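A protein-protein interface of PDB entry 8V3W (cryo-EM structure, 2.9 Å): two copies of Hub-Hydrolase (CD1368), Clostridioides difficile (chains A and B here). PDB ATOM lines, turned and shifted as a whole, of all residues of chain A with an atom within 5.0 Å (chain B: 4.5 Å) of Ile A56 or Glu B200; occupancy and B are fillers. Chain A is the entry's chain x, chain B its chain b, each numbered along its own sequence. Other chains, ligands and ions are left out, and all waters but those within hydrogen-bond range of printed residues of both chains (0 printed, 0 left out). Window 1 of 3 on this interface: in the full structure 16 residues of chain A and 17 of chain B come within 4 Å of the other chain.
Among the printed residues, pairs that only touch across the chains: Asn A76 with Glu B200 (3.6 Å), Ala A57 with Glu B230 (3.6 Å), Ile A75 with Ser B201 (3.7 Å), Ile A74 with Met B202 (3.8 Å), Ile A56 with Glu B200 (3.9 Å) and Ile A56 with Met B202 (3.9 Å).
No position is printed for both chains. Of the 10 pairs that touch across the chains among the printed residues, none has its exchanged pair printed and touching as well.
Printed residues of chain B that touch a printed residue of chain A: Ser B199, Glu B200, Ser B201, Met B202 and Glu B230. Among the printed residues, Asp or Glu carboxylates within 4 Å of a Lys or Arg side-chain nitrogen of the other chain: Arg A77 with Glu B200 (2.3 Å).
Ile A56 touches just these residues of chain B: Glu B200 and Met B202. Of the printed residues of chain B, Ala A57 touches Glu B230. Glu B200 touches just these residues of chain A: Ile A56 (3.9 Å), Asn A76 (3.6 Å) and Arg A77 (2.3 Å). Printed residues of chain A within 4 Å of Met B202: Ile A56 (3.9 Å), Ile A74 (3.8 Å) and Ile A75 (3.2 Å). The nearest residue of chain B that does not touch Ile A56 is Ile B256 (4.1 Å). The nearest residue of chain A that does not touch Glu B200 is Ile A75 (4.1 Å).
O of Ile A75 sits at hydrogen-bond distance from N of Met B202 (3.2 Å). The side-chain hydroxyl (OG) of Ser B201 is in hydrogen-bond range of the side-chain amide oxygen (OD1) of Asn A76 (2.8 Å). The backbone carbonyl oxygen (O) of Arg A77 sits at hydrogen-bond distance from the side-chain hydroxyl (OG) of Ser B199 (3.3 Å). The side-chain carboxylate (OE1) of Glu B200 is in salt-bridge range of the guanidinium group (NE) of Arg A77, 3.2 Å away.
O of Ile A54 lies within hydrogen-bond range of NH1 of Arg A77, at 3.3 Å. The backbone carbonyl oxygen (O) of Ile A74 is in hydrogen-bond range of the backbone NH (N) of Ala A57 (3.0 Å). O of Ser A58 sits at hydrogen-bond distance from N of Ile A74 (3.3 Å). The side-chain carboxylate of Glu B200 lies within salt-bridge range of the side-chain amino group of Lys B258 (3.2 Å). The backbone NH (N) of Ser B201 is in hydrogen-bond range of the backbone carbonyl oxygen (O) of Glu B257 (3.1 Å).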
ATOM      1  N   ILE A  54     -28.519  15.134  14.866  1.00  0.00           N
ATOM      2  CA  ILE A  54     -28.033  15.217  16.234  1.00  0.00           C
ATOM      3  C   ILE A  54     -26.801  16.111  16.239  1.00  0.00           C
ATOM      4  O   ILE A  54     -25.709  15.682  15.869  1.00  0.00           O
ATOM      5  CB  ILE A  54     -27.710  13.821  16.796  1.00  0.00           C
ATOM      6  CG1 ILE A  54     -28.931  12.916  16.680  1.00  0.00           C
ATOM      7  CG2 ILE A  54     -27.295  13.918  18.239  1.00  0.00           C
ATOM      8  CD1 ILE A  54     -28.613  11.455  16.818  1.00  0.00           C
ATOM      9  N   PRO A  55     -26.941  17.370  16.637  1.00  0.00           N
ATOM     10  CA  PRO A  55     -25.808  18.299  16.580  1.00  0.00           C
ATOM     11  C   PRO A  55     -24.750  17.979  17.625  1.00  0.00           C
ATOM     12  O   PRO A  55     -24.962  17.222  18.571  1.00  0.00           O
ATOM     13  CB  PRO A  55     -26.460  19.660  16.837  1.00  0.00           C
ATOM     14  CG  PRO A  55     -27.684  19.347  17.598  1.00  0.00           C
ATOM     15  CD  PRO A  55     -28.178  18.043  17.062  1.00  0.00           C
ATOM     16  N   ILE A  56     -23.577  18.582  17.423  1.00  0.00           N
ATOM     17  CA  ILE A  56     -22.467  18.420  18.350  1.00  0.00           C
ATOM     18  C   ILE A  56     -22.855  18.930  19.736  1.00  0.00           C
ATOM     19  O   ILE A  56     -23.634  19.879  19.880  1.00  0.00           O
ATOM     20  CB  ILE A  56     -21.231  19.157  17.803  1.00  0.00           C
ATOM     21  CG1 ILE A  56     -20.741  18.487  16.521  1.00  0.00           C
ATOM     22  CG2 ILE A  56     -20.118  19.240  18.830  1.00  0.00           C
ATOM     23  CD1 ILE A  56     -19.683  17.443  16.737  1.00  0.00           C
ATOM     24  N   ALA A  57     -22.323  18.267  20.767  1.00  0.00           N
ATOM     25  CA  ALA A  57     -22.469  18.677  22.164  1.00  0.00           C
ATOM     26  C   ALA A  57     -23.912  18.531  22.646  1.00  0.00           C
ATOM     27  O   ALA A  57     -24.459  19.413  23.304  1.00  0.00           O
ATOM     28  CB  ALA A  57     -21.957  20.103  22.383  1.00  0.00           C
ATOM     29  N   SER A  58     -24.518  17.395  22.324  1.00  0.00           N
ATOM     30  CA  SER A  58     -25.815  17.015  22.859  1.00  0.00           C
ATOM     31  C   SER A  58     -25.660  15.735  23.667  1.00  0.00           C
ATOM     32  O   SER A  58     -24.790  14.910  23.387  1.00  0.00           O
ATOM     33  CB  SER A  58     -26.848  16.822  21.747  1.00  0.00           C
ATOM     34  OG  SER A  58     -26.312  16.082  20.673  1.00  0.00           O
ATOM     35  N   ILE A  74     -21.561  14.542  22.969  1.00  0.00           N
ATOM     36  CA  ILE A  74     -21.144  14.167  21.621  1.00  0.00           C
ATOM     37  C   ILE A  74     -20.018  15.087  21.169  1.00  0.00           C
ATOM     38  O   ILE A  74     -20.130  16.314  21.253  1.00  0.00           O
ATOM     39  CB  ILE A  74     -22.337  14.216  20.656  1.00  0.00           C
ATOM     40  CG1 ILE A  74     -23.325  13.109  21.022  1.00  0.00           C
ATOM     41  CG2 ILE A  74     -21.875  14.085  19.223  1.00  0.00           C
ATOM     42  CD1 ILE A  74     -24.379  12.872  20.005  1.00  0.00           C
ATOM     43  N   ILE A  75     -18.924  14.496  20.684  1.00  0.00           N
ATOM     44  CA  ILE A  75     -17.698  15.226  20.400  1.00  0.00           C
ATOM     45  C   ILE A  75     -17.367  15.245  18.914  1.00  0.00           C
ATOM     46  O   ILE A  75     -16.991  16.289  18.374  1.00  0.00           O
ATOM     47  CB  ILE A  75     -16.518  14.654  21.212  1.00  0.00           C
ATOM     48  CG1 ILE A  75     -16.808  14.802  22.703  1.00  0.00           C
ATOM     49  CG2 ILE A  75     -15.222  15.348  20.836  1.00  0.00           C
ATOM     50  CD1 ILE A  75     -15.600  14.792  23.560  1.00  0.00           C
ATOM     51  N   ASN A  76     -17.509  14.114  18.229  1.00  0.00           N
ATOM     52  CA  ASN A  76     -17.202  14.010  16.812  1.00  0.00           C
ATOM     53  C   ASN A  76     -18.426  13.542  16.044  1.00  0.00           C
ATOM     54  O   ASN A  76     -19.284  12.839  16.581  1.00  0.00           O
ATOM     55  CB  ASN A  76     -16.048  13.039  16.549  1.00  0.00           C
ATOM     56  CG  ASN A  76     -14.703  13.640  16.850  1.00  0.00           C
ATOM     57  OD1 ASN A  76     -14.518  14.848  16.755  1.00  0.00           O
ATOM     58  ND2 ASN A  76     -13.747  12.797  17.203  1.00  0.00           N
ATOM     59  N   ARG A  77     -18.498  13.938  14.778  1.00  0.00           N
ATOM     60  CA  ARG A  77     -19.585  13.539  13.900  1.00  0.00           C
ATOM     61  C   ARG A  77     -19.050  13.452  12.479  1.00  0.00           C
ATOM     62  O   ARG A  77     -18.342  14.352  12.029  1.00  0.00           O
ATOM     63  CB  ARG A  77     -20.745  14.532  13.988  1.00  0.00           C
ATOM     64  CG  ARG A  77     -22.029  14.009  13.419  1.00  0.00           C
ATOM     65  CD  ARG A  77     -23.212  14.874  13.799  1.00  0.00           C
ATOM     66  NE  ARG A  77     -23.068  16.259  13.382  1.00  0.00           N
ATOM     67  CZ  ARG A  77     -24.059  16.995  12.901  1.00  0.00           C
ATOM     68  NH1 ARG A  77     -25.268  16.492  12.724  1.00  0.00           N
ATOM     69  NH2 ARG A  77     -23.831  18.264  12.585  1.00  0.00           N
ATOM     70  N   SER B 199     -17.117  16.106   8.113  1.00  0.00           N
ATOM     71  CA  SER B 199     -16.844  15.875   9.521  1.00  0.00           C
ATOM     72  C   SER B 199     -17.033  17.161  10.310  1.00  0.00           C
ATOM     73  O   SER B 199     -16.940  18.262   9.766  1.00  0.00           O
ATOM     74  CB  SER B 199     -15.425  15.343   9.729  1.00  0.00           C
ATOM     75  OG  SER B 199     -15.269  14.806  11.027  1.00  0.00           O
ATOM     76  N   GLU B 200     -17.312  17.002  11.600  1.00  0.00           N
ATOM     77  CA  GLU B 200     -17.374  18.097  12.554  1.00  0.00           C
ATOM     78  C   GLU B 200     -16.718  17.643  13.849  1.00  0.00           C
ATOM     79  O   GLU B 200     -16.870  16.489  14.251  1.00  0.00           O
ATOM     80  CB  GLU B 200     -18.814  18.528  12.823  1.00  0.00           C
ATOM     81  CG  GLU B 200     -19.356  19.517  11.831  1.00  0.00           C
ATOM     82  CD  GLU B 200     -20.810  19.829  12.076  1.00  0.00           C
ATOM     83  OE1 GLU B 200     -21.589  18.882  12.296  1.00  0.00           O
ATOM     84  OE2 GLU B 200     -21.180  21.021  12.047  1.00  0.00           O
ATOM     85  N   SER B 201     -15.986  18.544  14.498  1.00  0.00           N
ATOM     86  CA  SER B 201     -15.221  18.174  15.675  1.00  0.00           C
ATOM     87  C   SER B 201     -15.276  19.283  16.712  1.00  0.00           C
ATOM     88  O   SER B 201     -15.432  20.459  16.382  1.00  0.00           O
ATOM     89  CB  SER B 201     -13.765  17.862  15.323  1.00  0.00           C
ATOM     90  OG  SER B 201     -13.116  17.204  16.391  1.00  0.00           O
ATOM     91  N   MET B 202     -15.118  18.890  17.972  1.00  0.00           N
ATOM     92  CA  MET B 202     -15.184  19.791  19.111  1.00  0.00           C
ATOM     93  C   MET B 202     -13.883  19.792  19.909  1.00  0.00           C
ATOM     94  O   MET B 202     -13.746  20.569  20.859  1.00  0.00           O
ATOM     95  CB  MET B 202     -16.392  19.390  19.979  1.00  0.00           C
ATOM     96  CG  MET B 202     -16.457  19.875  21.407  1.00  0.00           C
ATOM     97  SD  MET B 202     -17.856  19.177  22.293  1.00  0.00           S
ATOM     98  CE  MET B 202     -17.177  19.082  23.938  1.00  0.00           C
ATOM     99  N   GLU B 230     -23.009  27.019  22.006  1.00  0.00           N
ATOM    100  CA  GLU B 230     -22.935  25.743  21.304  1.00  0.00           C
ATOM    101  C   GLU B 230     -22.474  24.622  22.226  1.00  0.00           C
ATOM    102  O   GLU B 230     -23.030  23.519  22.189  1.00  0.00           O
ATOM    103  CB  GLU B 230     -22.006  25.866  20.101  1.00  0.00           C
ATOM    104  CG  GLU B 230     -22.610  26.635  18.945  1.00  0.00           C
ATOM    105  CD  GLU B 230     -21.588  27.465  18.196  1.00  0.00           C
ATOM    106  OE1 GLU B 230     -20.517  26.925  17.848  1.00  0.00           O
ATOM    107  OE2 GLU B 230     -21.857  28.661  17.957  1.00  0.00           O
ATOM    108  N   ILE B 256     -15.955  25.494  16.646  1.00  0.00           N
ATOM    109  CA  ILE B 256     -16.085  24.161  16.073  1.00  0.00           C
ATOM    110  C   ILE B 256     -15.498  24.139  14.668  1.00  0.00           C
ATOM    111  O   ILE B 256     -15.666  25.087  13.889  1.00  0.00           O
ATOM    112  CB  ILE B 256     -17.564  23.733  16.073  1.00  0.00           C
ATOM    113  CG1 ILE B 256     -18.103  23.685  17.500  1.00  0.00           C
ATOM    114  CG2 ILE B 256     -17.746  22.385  15.412  1.00  0.00           C
ATOM    115  CD1 ILE B 256     -19.472  23.076  17.608  1.00  0.00           C
ATOM    116  N   GLU B 257     -14.807  23.052  14.333  1.00  0.00           N
ATOM    117  CA  GLU B 257     -14.165  22.896  13.036  1.00  0.00           C
ATOM    118  C   GLU B 257     -14.985  21.967  12.155  1.00  0.00           C
ATOM    119  O   GLU B 257     -15.378  20.881  12.588  1.00  0.00           O
ATOM    120  CB  GLU B 257     -12.748  22.348  13.193  1.00  0.00           C
ATOM    121  CG  GLU B 257     -11.900  23.130  14.169  1.00  0.00           C
ATOM    122  CD  GLU B 257     -10.441  22.735  14.118  1.00  0.00           C
ATOM    123  OE1 GLU B 257     -10.133  21.661  13.561  1.00  0.00           O
ATOM    124  OE2 GLU B 257      -9.600  23.504  14.628  1.00  0.00           O
ATOM    125  N   LYS B 258     -15.234  22.394  10.921  1.00  0.00           N
ATOM    126  CA  LYS B 258     -15.994  21.624   9.946  1.00  0.00           C
ATOM    127  C   LYS B 258     -15.153  21.456   8.690  1.00  0.00           C
ATOM    128  O   LYS B 258     -14.596  22.432   8.182  1.00  0.00           O
ATOM    129  CB  LYS B 258     -17.315  22.314   9.623  1.00  0.00           C
ATOM    130  CG  LYS B 258     -18.033  22.855  10.841  1.00  0.00           C
ATOM    131  CD  LYS B 258     -18.864  24.063  10.486  1.00  0.00           C
ATOM    132  CE  LYS B 258     -19.274  24.835  11.723  1.00  0.00           C
ATOM    133  NZ  LYS B 258     -20.070  23.998  12.650  1.00  0.00           N
